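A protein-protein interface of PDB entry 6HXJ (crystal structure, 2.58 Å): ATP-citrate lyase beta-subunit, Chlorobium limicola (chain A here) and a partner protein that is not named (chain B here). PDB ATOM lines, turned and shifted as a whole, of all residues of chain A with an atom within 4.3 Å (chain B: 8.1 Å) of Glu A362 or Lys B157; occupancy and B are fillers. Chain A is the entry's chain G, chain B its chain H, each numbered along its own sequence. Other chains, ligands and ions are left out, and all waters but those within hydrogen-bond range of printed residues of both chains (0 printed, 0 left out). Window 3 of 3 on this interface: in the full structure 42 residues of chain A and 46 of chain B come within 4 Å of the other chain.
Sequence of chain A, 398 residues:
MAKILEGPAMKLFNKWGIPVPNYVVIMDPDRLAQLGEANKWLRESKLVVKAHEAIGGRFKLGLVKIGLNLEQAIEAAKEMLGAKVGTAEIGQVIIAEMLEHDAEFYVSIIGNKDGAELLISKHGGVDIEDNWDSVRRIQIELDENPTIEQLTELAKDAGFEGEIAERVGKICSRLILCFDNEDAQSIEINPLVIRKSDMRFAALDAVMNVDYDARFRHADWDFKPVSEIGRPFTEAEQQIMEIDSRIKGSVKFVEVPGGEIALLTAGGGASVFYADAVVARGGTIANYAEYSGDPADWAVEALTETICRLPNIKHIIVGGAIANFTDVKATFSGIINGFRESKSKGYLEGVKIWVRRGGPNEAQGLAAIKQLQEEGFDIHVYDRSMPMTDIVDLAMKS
Among the printed residues, merely in contact across the chains: Glu A362 with Lys B157, Arg A384 with Leu B161, Pro A360 with Glu B155 and Pro A360 with Arg B25.
The side-chain carboxylate (OE1) of Glu B155 sits at hydrogen-bond distance from the backbone NH (N) of Asn A361. OD1 of Asn B158 lies within hydrogen-bond range of NH2 of Arg A384, 2.5 Å away. The side-chain sulfur of Cys B162 lies within hydrogen-bond range of the guanidinium group of Arg A384 (3.6 Å). The backbone carbonyl oxygen (O) of Arg A384 lies within hydrogen-bond range of the indole nitrogen (NE1) of Trp B185 (3.2 Å). The backbone carbonyl oxygen (O) of Gly A359 sits close to the side-chain carboxylate (OE2) of Glu B155 (3.4 Å). The side-chain carboxylate of Glu A362 sits close to the side-chain carboxylate of Glu B155 (3.4 Å).
N of Val A328 sits at hydrogen-bond distance from O of Pro A360 (2.8 Å). The side-chain amide oxygen (OD1) of Asn A361 lies within hydrogen-bond range of the side-chain amide nitrogen (NE2) of Gln A364 (2.9 Å). OE1 of Glu A362 lies within salt-bridge range of NH1 of Arg A384. O of Gly B153 lies within hydrogen-bond range of ND2 of Asn B158 (2.7 Å). The side-chain sulfur (SG) of Cys B162 sits close to the backbone carbonyl oxygen (O) of Asn B158 (3.4 Å). ND2 of Asn B158 lies within hydrogen-bond range of OD1 of Asn B181 (2.9 Å).
Of the 20 printed residues of chain B, 7 touch a printed residue of chain A. Hydrophobic or aromatic side chains of chain B that line the printed part of chain A: Leu B161 and Trp B185. Of the 12 printed residues of chain A, 5 touch a printed residue of chain B. Hydrophobic or aromatic side chains of chain A that line the printed part of chain B: Pro A360. Among the printed residues, no Asp or Glu carboxylate lies within 4 Å of a Lys or Arg side-chain nitrogen of the other chain.
Gly A359 touches just one residue of chain B: Glu B155. Printed residues of chain B within 4 Å of Asn A361: Glu B155 (3.3 Å). Of the printed residues of chain B, Glu A362 touches Glu B155 and Lys B157. No residue of chain B comes within 4 Å of Ala A363. Printed residues of chain A within 4 Å of Arg B25: Pro A360. Gln B28 touches none of the printed residues of chain A. Lys B157 touches one residue of chain A. Printed residues of chain A within 4 Å of Cys B162: Arg A384. Printed residues of chain A within 4 Å of Trp B185: Arg A384 (3.2 Å). The nearest residue of chain B that does not touch Glu A362 is Asn B158 (4.9 Å). The nearest printed residue of chain A that does not touch Asn B158 is Glu A362 (4.9 Å).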
ATOM      1  N   VAL A 328      18.307 -28.095 -25.700  1.00  0.00           N
ATOM      2  CA  VAL A 328      17.820 -26.719 -25.639  1.00  0.00           C
ATOM      3  C   VAL A 328      16.733 -26.484 -26.731  1.00  0.00           C
ATOM      4  O   VAL A 328      15.841 -25.676 -26.487  1.00  0.00           O
ATOM      5  CB  VAL A 328      18.910 -25.601 -25.565  1.00  0.00           C
ATOM      6  CG1 VAL A 328      20.021 -25.937 -24.581  1.00  0.00           C
ATOM      7  CG2 VAL A 328      19.469 -25.220 -26.921  1.00  0.00           C
ATOM      8  N   ARG A 357      21.832 -18.827 -23.501  1.00  0.00           N
ATOM      9  CA  ARG A 357      21.860 -20.274 -23.336  1.00  0.00           C
ATOM     10  C   ARG A 357      22.868 -20.979 -24.250  1.00  0.00           C
ATOM     11  O   ARG A 357      23.241 -20.470 -25.308  1.00  0.00           O
ATOM     12  CB  ARG A 357      20.417 -20.842 -23.530  1.00  0.00           C
ATOM     13  CG  ARG A 357      20.185 -22.316 -23.191  1.00  0.00           C
ATOM     14  CD  ARG A 357      20.400 -22.631 -21.725  1.00  0.00           C
ATOM     15  NE  ARG A 357      19.820 -23.919 -21.373  1.00  0.00           N
ATOM     16  CZ  ARG A 357      20.407 -24.798 -20.572  1.00  0.00           C
ATOM     17  NH1 ARG A 357      21.588 -24.525 -20.029  1.00  0.00           N
ATOM     18  NH2 ARG A 357      19.809 -25.950 -20.290  1.00  0.00           N
ATOM     19  N   GLY A 358      23.300 -22.143 -23.783  1.00  0.00           N
ATOM     20  CA  GLY A 358      24.193 -23.065 -24.464  1.00  0.00           C
ATOM     21  C   GLY A 358      23.785 -24.484 -24.119  1.00  0.00           C
ATOM     22  O   GLY A 358      23.050 -24.703 -23.137  1.00  0.00           O
ATOM     23  N   GLY A 359      24.276 -25.448 -24.903  1.00  0.00           N
ATOM     24  CA  GLY A 359      23.988 -26.864 -24.686  1.00  0.00           C
ATOM     25  C   GLY A 359      23.556 -27.594 -25.939  1.00  0.00           C
ATOM     26  O   GLY A 359      23.590 -26.989 -27.012  1.00  0.00           O
ATOM     27  N   PRO A 360      23.140 -28.894 -25.848  1.00  0.00           N
ATOM     28  CA  PRO A 360      22.772 -29.648 -27.071  1.00  0.00           C
ATOM     29  C   PRO A 360      21.593 -29.055 -27.838  1.00  0.00           C
ATOM     30  O   PRO A 360      20.552 -28.763 -27.253  1.00  0.00           O
ATOM     31  CB  PRO A 360      22.509 -31.059 -26.550  1.00  0.00           C
ATOM     32  CG  PRO A 360      23.266 -31.133 -25.252  1.00  0.00           C
ATOM     33  CD  PRO A 360      23.094 -29.769 -24.661  1.00  0.00           C
ATOM     34  N   ASN A 361      21.810 -28.807 -29.146  1.00  0.00           N
ATOM     35  CA  ASN A 361      20.892 -28.173 -30.100  1.00  0.00           C
ATOM     36  C   ASN A 361      20.654 -26.694 -29.768  1.00  0.00           C
ATOM     37  O   ASN A 361      19.542 -26.188 -29.949  1.00  0.00           O
ATOM     38  CB  ASN A 361      19.592 -28.960 -30.284  1.00  0.00           C
ATOM     39  CG  ASN A 361      19.825 -30.258 -30.995  1.00  0.00           C
ATOM     40  OD1 ASN A 361      20.162 -30.289 -32.181  1.00  0.00           O
ATOM     41  ND2 ASN A 361      19.713 -31.357 -30.278  1.00  0.00           N
ATOM     42  N   GLU A 362      21.733 -25.989 -29.328  1.00  0.00           N
ATOM     43  CA  GLU A 362      21.691 -24.572 -28.999  1.00  0.00           C
ATOM     44  C   GLU A 362      21.435 -23.714 -30.211  1.00  0.00           C
ATOM     45  O   GLU A 362      20.696 -22.745 -30.083  1.00  0.00           O
ATOM     46  CB  GLU A 362      22.911 -24.079 -28.193  1.00  0.00           C
ATOM     47  CG  GLU A 362      24.284 -24.230 -28.837  1.00  0.00           C
ATOM     48  CD  GLU A 362      25.430 -23.845 -27.915  1.00  0.00           C
ATOM     49  OE1 GLU A 362      26.067 -24.756 -27.335  1.00  0.00           O
ATOM     50  OE2 GLU A 362      25.672 -22.628 -27.747  1.00  0.00           O
ATOM     51  N   ALA A 363      21.990 -24.076 -31.388  1.00  0.00           N
ATOM     52  CA  ALA A 363      21.800 -23.320 -32.626  1.00  0.00           C
ATOM     53  C   ALA A 363      20.312 -23.188 -32.973  1.00  0.00           C
ATOM     54  O   ALA A 363      19.813 -22.067 -33.069  1.00  0.00           O
ATOM     55  CB  ALA A 363      22.554 -23.984 -33.759  1.00  0.00           C
ATOM     56  N   GLN A 364      19.599 -24.336 -33.065  1.00  0.00           N
ATOM     57  CA  GLN A 364      18.164 -24.435 -33.362  1.00  0.00           C
ATOM     58  C   GLN A 364      17.307 -23.769 -32.280  1.00  0.00           C
ATOM     59  O   GLN A 364      16.369 -23.040 -32.599  1.00  0.00           O
ATOM     60  CB  GLN A 364      17.735 -25.902 -33.531  1.00  0.00           C
ATOM     61  CG  GLN A 364      18.398 -26.626 -34.695  1.00  0.00           C
ATOM     62  CD  GLN A 364      19.426 -27.628 -34.232  1.00  0.00           C
ATOM     63  OE1 GLN A 364      20.430 -27.286 -33.581  1.00  0.00           O
ATOM     64  NE2 GLN A 364      19.206 -28.889 -34.585  1.00  0.00           N
ATOM     65  N   GLY A 365      17.651 -24.029 -31.023  1.00  0.00           N
ATOM     66  CA  GLY A 365      16.955 -23.498 -29.862  1.00  0.00           C
ATOM     67  C   GLY A 365      16.997 -21.991 -29.775  1.00  0.00           C
ATOM     68  O   GLY A 365      15.955 -21.349 -29.598  1.00  0.00           O
ATOM     69  N   LEU A 366      18.208 -21.420 -29.912  1.00  0.00           N
ATOM     70  CA  LEU A 366      18.442 -19.979 -29.846  1.00  0.00           C
ATOM     71  C   LEU A 366      17.878 -19.242 -31.063  1.00  0.00           C
ATOM     72  O   LEU A 366      17.451 -18.095 -30.923  1.00  0.00           O
ATOM     73  CB  LEU A 366      19.937 -19.651 -29.610  1.00  0.00           C
ATOM     74  CG  LEU A 366      20.478 -19.510 -28.154  1.00  0.00           C
ATOM     75  CD1 LEU A 366      19.862 -18.333 -27.408  1.00  0.00           C
ATOM     76  CD2 LEU A 366      20.347 -20.793 -27.337  1.00  0.00           C
ATOM     77  N   ARG A 384      26.689 -18.210 -26.020  1.00  0.00           N
ATOM     78  CA  ARG A 384      27.791 -18.422 -25.069  1.00  0.00           C
ATOM     79  C   ARG A 384      28.830 -17.287 -24.983  1.00  0.00           C
ATOM     80  O   ARG A 384      29.433 -17.108 -23.922  1.00  0.00           O
ATOM     81  CB  ARG A 384      28.494 -19.742 -25.382  1.00  0.00           C
ATOM     82  CG  ARG A 384      28.924 -19.852 -26.832  1.00  0.00           C
ATOM     83  CD  ARG A 384      28.931 -21.287 -27.246  1.00  0.00           C
ATOM     84  NE  ARG A 384      29.992 -21.980 -26.537  1.00  0.00           N
ATOM     85  CZ  ARG A 384      29.931 -23.229 -26.115  1.00  0.00           C
ATOM     86  NH1 ARG A 384      28.851 -23.973 -26.361  1.00  0.00           N
ATOM     87  NH2 ARG A 384      30.958 -23.760 -25.468  1.00  0.00           N
ATOM     88  N   ARG B  25      28.182 -40.521 -25.661  1.00  0.00           N
ATOM     89  CA  ARG B  25      28.885 -39.242 -25.505  1.00  0.00           C
ATOM     90  C   ARG B  25      30.385 -39.472 -25.292  1.00  0.00           C
ATOM     91  O   ARG B  25      31.204 -38.793 -25.913  1.00  0.00           O
ATOM     92  CB  ARG B  25      28.296 -38.405 -24.354  1.00  0.00           C
ATOM     93  CG  ARG B  25      27.002 -37.699 -24.726  1.00  0.00           C
ATOM     94  CD  ARG B  25      27.196 -36.686 -25.841  1.00  0.00           C
ATOM     95  NE  ARG B  25      26.085 -35.732 -25.924  1.00  0.00           N
ATOM     96  CZ  ARG B  25      25.630 -35.196 -27.050  1.00  0.00           C
ATOM     97  NH1 ARG B  25      26.158 -35.541 -28.220  1.00  0.00           N
ATOM     98  NH2 ARG B  25      24.636 -34.322 -27.020  1.00  0.00           N
ATOM     99  N   GLN B  28      32.137 -40.269 -28.534  1.00  0.00           N
ATOM    100  CA  GLN B  28      32.323 -39.055 -29.332  1.00  0.00           C
ATOM    101  C   GLN B  28      33.636 -38.374 -28.914  1.00  0.00           C
ATOM    102  O   GLN B  28      34.387 -37.872 -29.770  1.00  0.00           O
ATOM    103  CB  GLN B  28      31.157 -38.084 -29.101  1.00  0.00           C
ATOM    104  CG  GLN B  28      30.099 -38.219 -30.153  1.00  0.00           C
ATOM    105  CD  GLN B  28      28.846 -37.459 -29.878  1.00  0.00           C
ATOM    106  OE1 GLN B  28      28.557 -37.065 -28.766  1.00  0.00           O
ATOM    107  NE2 GLN B  28      28.011 -37.336 -30.878  1.00  0.00           N
ATOM    108  N   LEU B  32      37.257 -37.912 -30.970  1.00  0.00           N
ATOM    109  CA  LEU B  32      37.900 -36.600 -31.017  1.00  0.00           C
ATOM    110  C   LEU B  32      39.386 -36.613 -30.580  1.00  0.00           C
ATOM    111  O   LEU B  32      40.223 -35.995 -31.231  1.00  0.00           O
ATOM    112  CB  LEU B  32      37.101 -35.598 -30.162  1.00  0.00           C
ATOM    113  CG  LEU B  32      37.673 -34.185 -29.999  1.00  0.00           C
ATOM    114  CD1 LEU B  32      37.548 -33.354 -31.311  1.00  0.00           C
ATOM    115  CD2 LEU B  32      37.029 -33.494 -28.833  1.00  0.00           C
ATOM    116  N   GLY B 153      30.439 -31.982 -20.609  1.00  0.00           N
ATOM    117  CA  GLY B 153      31.015 -31.414 -21.820  1.00  0.00           C
ATOM    118  C   GLY B 153      30.033 -31.205 -22.956  1.00  0.00           C
ATOM    119  O   GLY B 153      30.394 -30.578 -23.955  1.00  0.00           O
ATOM    120  N   GLY B 154      28.825 -31.779 -22.840  1.00  0.00           N
ATOM    121  CA  GLY B 154      27.738 -31.652 -23.820  1.00  0.00           C
ATOM    122  C   GLY B 154      27.973 -32.161 -25.224  1.00  0.00           C
ATOM    123  O   GLY B 154      28.623 -33.183 -25.403  1.00  0.00           O
ATOM    124  N   GLU B 155      27.417 -31.450 -26.231  1.00  0.00           N
ATOM    125  CA  GLU B 155      27.510 -31.797 -27.662  1.00  0.00           C
ATOM    126  C   GLU B 155      28.953 -31.693 -28.215  1.00  0.00           C
ATOM    127  O   GLU B 155      29.802 -30.990 -27.633  1.00  0.00           O
ATOM    128  CB  GLU B 155      26.499 -30.990 -28.511  1.00  0.00           C
ATOM    129  CG  GLU B 155      26.860 -29.534 -28.785  1.00  0.00           C
ATOM    130  CD  GLU B 155      25.833 -28.682 -29.518  1.00  0.00           C
ATOM    131  OE1 GLU B 155      24.924 -29.246 -30.172  1.00  0.00           O
ATOM    132  OE2 GLU B 155      25.937 -27.435 -29.429  1.00  0.00           O
ATOM    133  N   PHE B 156      29.224 -32.418 -29.328  1.00  0.00           N
ATOM    134  CA  PHE B 156      30.544 -32.473 -29.944  1.00  0.00           C
ATOM    135  C   PHE B 156      31.127 -31.083 -30.282  1.00  0.00           C
ATOM    136  O   PHE B 156      32.316 -30.837 -30.026  1.00  0.00           O
ATOM    137  CB  PHE B 156      30.529 -33.396 -31.155  1.00  0.00           C
ATOM    138  CG  PHE B 156      31.881 -33.775 -31.724  1.00  0.00           C
ATOM    139  CD1 PHE B 156      32.613 -34.822 -31.178  1.00  0.00           C
ATOM    140  CD2 PHE B 156      32.396 -33.114 -32.831  1.00  0.00           C
ATOM    141  CE1 PHE B 156      33.841 -35.198 -31.729  1.00  0.00           C
ATOM    142  CE2 PHE B 156      33.615 -33.492 -33.384  1.00  0.00           C
ATOM    143  CZ  PHE B 156      34.328 -34.536 -32.836  1.00  0.00           C
ATOM    144  N   LYS B 157      30.280 -30.164 -30.798  1.00  0.00           N
ATOM    145  CA  LYS B 157      30.637 -28.770 -31.110  1.00  0.00           C
ATOM    146  C   LYS B 157      31.194 -28.054 -29.825  1.00  0.00           C
ATOM    147  O   LYS B 157      32.137 -27.243 -29.915  1.00  0.00           O
ATOM    148  CB  LYS B 157      29.397 -28.051 -31.677  1.00  0.00           C
ATOM    149  CG  LYS B 157      29.525 -26.543 -31.888  1.00  0.00           C
ATOM    150  CD  LYS B 157      28.333 -25.814 -31.252  1.00  0.00           C
ATOM    151  CE  LYS B 157      27.973 -24.523 -31.942  1.00  0.00           C
ATOM    152  NZ  LYS B 157      26.695 -23.965 -31.421  1.00  0.00           N
ATOM    153  N   ASN B 158      30.639 -28.403 -28.637  1.00  0.00           N
ATOM    154  CA  ASN B 158      31.094 -27.841 -27.381  1.00  0.00           C
ATOM    155  C   ASN B 158      32.476 -28.344 -27.005  1.00  0.00           C
ATOM    156  O   ASN B 158      33.285 -27.565 -26.491  1.00  0.00           O
ATOM    157  CB  ASN B 158      30.094 -28.113 -26.280  1.00  0.00           C
ATOM    158  CG  ASN B 158      30.394 -27.314 -25.050  1.00  0.00           C
ATOM    159  OD1 ASN B 158      30.188 -26.122 -25.016  1.00  0.00           O
ATOM    160  ND2 ASN B 158      30.927 -27.938 -24.032  1.00  0.00           N
ATOM    161  N   LEU B 159      32.766 -29.630 -27.275  1.00  0.00           N
ATOM    162  CA  LEU B 159      34.096 -30.198 -26.993  1.00  0.00           C
ATOM    163  C   LEU B 159      35.177 -29.417 -27.752  1.00  0.00           C
ATOM    164  O   LEU B 159      36.269 -29.189 -27.219  1.00  0.00           O
ATOM    165  CB  LEU B 159      34.188 -31.676 -27.397  1.00  0.00           C
ATOM    166  CG  LEU B 159      33.214 -32.676 -26.777  1.00  0.00           C
ATOM    167  CD1 LEU B 159      33.542 -34.093 -27.271  1.00  0.00           C
ATOM    168  CD2 LEU B 159      33.204 -32.601 -25.222  1.00  0.00           C
ATOM    169  N   LYS B 160      34.846 -28.989 -28.987  1.00  0.00           N
ATOM    170  CA  LYS B 160      35.727 -28.227 -29.862  1.00  0.00           C
ATOM    171  C   LYS B 160      35.860 -26.771 -29.415  1.00  0.00           C
ATOM    172  O   LYS B 160      36.982 -26.251 -29.375  1.00  0.00           O
ATOM    173  CB  LYS B 160      35.257 -28.343 -31.314  1.00  0.00           C
ATOM    174  CG  LYS B 160      35.584 -29.695 -31.928  1.00  0.00           C
ATOM    175  CD  LYS B 160      35.179 -29.749 -33.361  1.00  0.00           C
ATOM    176  CE  LYS B 160      36.043 -30.727 -34.099  1.00  0.00           C
ATOM    177  NZ  LYS B 160      35.733 -30.750 -35.555  1.00  0.00           N
ATOM    178  N   LEU B 161      34.729 -26.129 -29.036  1.00  0.00           N
ATOM    179  CA  LEU B 161      34.707 -24.749 -28.537  1.00  0.00           C
ATOM    180  C   LEU B 161      35.461 -24.580 -27.216  1.00  0.00           C
ATOM    181  O   LEU B 161      36.042 -23.522 -26.980  1.00  0.00           O
ATOM    182  CB  LEU B 161      33.267 -24.253 -28.364  1.00  0.00           C
ATOM    183  CG  LEU B 161      32.550 -23.841 -29.635  1.00  0.00           C
ATOM    184  CD1 LEU B 161      31.056 -23.872 -29.445  1.00  0.00           C
ATOM    185  CD2 LEU B 161      32.963 -22.474 -30.059  1.00  0.00           C
ATOM    186  N   CYS B 162      35.429 -25.607 -26.353  1.00  0.00           N
ATOM    187  CA  CYS B 162      36.096 -25.581 -25.049  1.00  0.00           C
ATOM    188  C   CYS B 162      37.518 -26.155 -25.111  1.00  0.00           C
ATOM    189  O   CYS B 162      38.178 -26.284 -24.072  1.00  0.00           O
ATOM    190  CB  CYS B 162      35.246 -26.276 -23.987  1.00  0.00           C
ATOM    191  SG  CYS B 162      33.618 -25.535 -23.744  1.00  0.00           S
ATOM    192  N   ASN B 163      37.975 -26.508 -26.337  1.00  0.00           N
ATOM    193  CA  ASN B 163      39.305 -27.056 -26.628  1.00  0.00           C
ATOM    194  C   ASN B 163      39.629 -28.293 -25.790  1.00  0.00           C
ATOM    195  O   ASN B 163      40.775 -28.489 -25.347  1.00  0.00           O
ATOM    196  CB  ASN B 163      40.395 -25.971 -26.472  1.00  0.00           C
ATOM    197  CG  ASN B 163      40.208 -24.791 -27.377  1.00  0.00           C
ATOM    198  OD1 ASN B 163      40.067 -24.916 -28.605  1.00  0.00           O
ATOM    199  ND2 ASN B 163      40.184 -23.622 -26.776  1.00  0.00           N
ATOM    200  N   LEU B 164      38.610 -29.154 -25.614  1.00  0.00           N
ATOM    201  CA  LEU B 164      38.704 -30.345 -24.772  1.00  0.00           C
ATOM    202  C   LEU B 164      39.498 -31.482 -25.420  1.00  0.00           C
ATOM    203  O   LEU B 164      39.627 -32.552 -24.831  1.00  0.00           O
ATOM    204  CB  LEU B 164      37.301 -30.781 -24.312  1.00  0.00           C
ATOM    205  CG  LEU B 164      36.509 -29.714 -23.541  1.00  0.00           C
ATOM    206  CD1 LEU B 164      35.162 -30.215 -23.143  1.00  0.00           C
ATOM    207  CD2 LEU B 164      37.271 -29.223 -22.303  1.00  0.00           C
ATOM    208  N   TYR B 165      40.087 -31.220 -26.590  1.00  0.00           N
ATOM    209  CA  TYR B 165      40.913 -32.179 -27.319  1.00  0.00           C
ATOM    210  C   TYR B 165      42.401 -32.094 -26.912  1.00  0.00           C
ATOM    211  O   TYR B 165      43.210 -32.850 -27.439  1.00  0.00           O
ATOM    212  CB  TYR B 165      40.753 -31.983 -28.833  1.00  0.00           C
ATOM    213  CG  TYR B 165      40.965 -30.554 -29.288  1.00  0.00           C
ATOM    214  CD1 TYR B 165      39.903 -29.648 -29.326  1.00  0.00           C
ATOM    215  CD2 TYR B 165      42.222 -30.106 -29.691  1.00  0.00           C
ATOM    216  CE1 TYR B 165      40.088 -28.334 -29.752  1.00  0.00           C
ATOM    217  CE2 TYR B 165      42.414 -28.800 -30.140  1.00  0.00           C
ATOM    218  CZ  TYR B 165      41.344 -27.917 -30.157  1.00  0.00           C
ATOM    219  OH  TYR B 165      41.505 -26.619 -30.571  1.00  0.00           O
ATOM    220  N   ASN B 181      30.504 -27.163 -17.115  1.00  0.00           N
ATOM    221  CA  ASN B 181      30.513 -26.877 -18.545  1.00  0.00           C
ATOM    222  C   ASN B 181      30.740 -25.366 -18.813  1.00  0.00           C
ATOM    223  O   ASN B 181      31.458 -25.011 -19.742  1.00  0.00           O
ATOM    224  CB  ASN B 181      29.221 -27.385 -19.185  1.00  0.00           C
ATOM    225  CG  ASN B 181      29.387 -27.886 -20.589  1.00  0.00           C
ATOM    226  OD1 ASN B 181      30.486 -27.896 -21.153  1.00  0.00           O
ATOM    227  ND2 ASN B 181      28.292 -28.304 -21.193  1.00  0.00           N
ATOM    228  N   TRP B 185      34.266 -23.625 -20.461  1.00  0.00           N
ATOM    229  CA  TRP B 185      34.158 -22.635 -21.517  1.00  0.00           C
ATOM    230  C   TRP B 185      34.930 -21.370 -21.150  1.00  0.00           C
ATOM    231  O   TRP B 185      35.636 -20.825 -21.998  1.00  0.00           O
ATOM    232  CB  TRP B 185      32.687 -22.321 -21.798  1.00  0.00           C
ATOM    233  CG  TRP B 185      32.478 -21.040 -22.554  1.00  0.00           C
ATOM    234  CD1 TRP B 185      31.842 -19.921 -22.107  1.00  0.00           C
ATOM    235  CD2 TRP B 185      32.947 -20.733 -23.879  1.00  0.00           C
ATOM    236  NE1 TRP B 185      31.873 -18.937 -23.074  1.00  0.00           N
ATOM    237  CE2 TRP B 185      32.544 -19.409 -24.172  1.00  0.00           C
ATOM    238  CE3 TRP B 185      33.677 -21.449 -24.850  1.00  0.00           C
ATOM    239  CZ2 TRP B 185      32.829 -18.792 -25.398  1.00  0.00           C
ATOM    240  CZ3 TRP B 185      33.949 -20.841 -26.064  1.00  0.00           C
ATOM    241  CH2 TRP B 185      33.530 -19.527 -26.327  1.00  0.00           C
ATOM    242  N   GLU B 335      36.080 -34.368 -37.526  1.00  0.00           N
ATOM    243  CA  GLU B 335      34.702 -33.902 -37.464  1.00  0.00           C
ATOM    244  C   GLU B 335      33.776 -35.123 -37.446  1.00  0.00           C
ATOM    245  O   GLU B 335      34.103 -36.143 -38.043  1.00  0.00           O
ATOM    246  CB  GLU B 335      34.372 -32.889 -38.584  1.00  0.00           C
ATOM    247  CG  GLU B 335      33.017 -32.181 -38.429  1.00  0.00           C
ATOM    248  CD  GLU B 335      32.498 -31.865 -37.026  1.00  0.00           C
ATOM    249  OE1 GLU B 335      31.498 -32.491 -36.598  1.00  0.00           O
ATOM    250  OE2 GLU B 335      33.094 -30.992 -36.354  1.00  0.00           O
ATOM    251  N   LEU B 336      32.684 -35.061 -36.697  1.00  0.00           N
ATOM    252  CA  LEU B 336      31.772 -36.190 -36.613  1.00  0.00           C
ATOM    253  C   LEU B 336      31.244 -36.505 -37.966  1.00  0.00           C
ATOM    254  O   LEU B 336      30.867 -35.567 -38.664  1.00  0.00           O
ATOM    255  CB  LEU B 336      30.582 -35.885 -35.708  1.00  0.00           C
ATOM    256  CG  LEU B 336      30.742 -36.086 -34.228  1.00  0.00           C
ATOM    257  CD1 LEU B 336      29.400 -36.013 -33.585  1.00  0.00           C
ATOM    258  CD2 LEU B 336      31.405 -37.413 -33.897  1.00  0.00           C
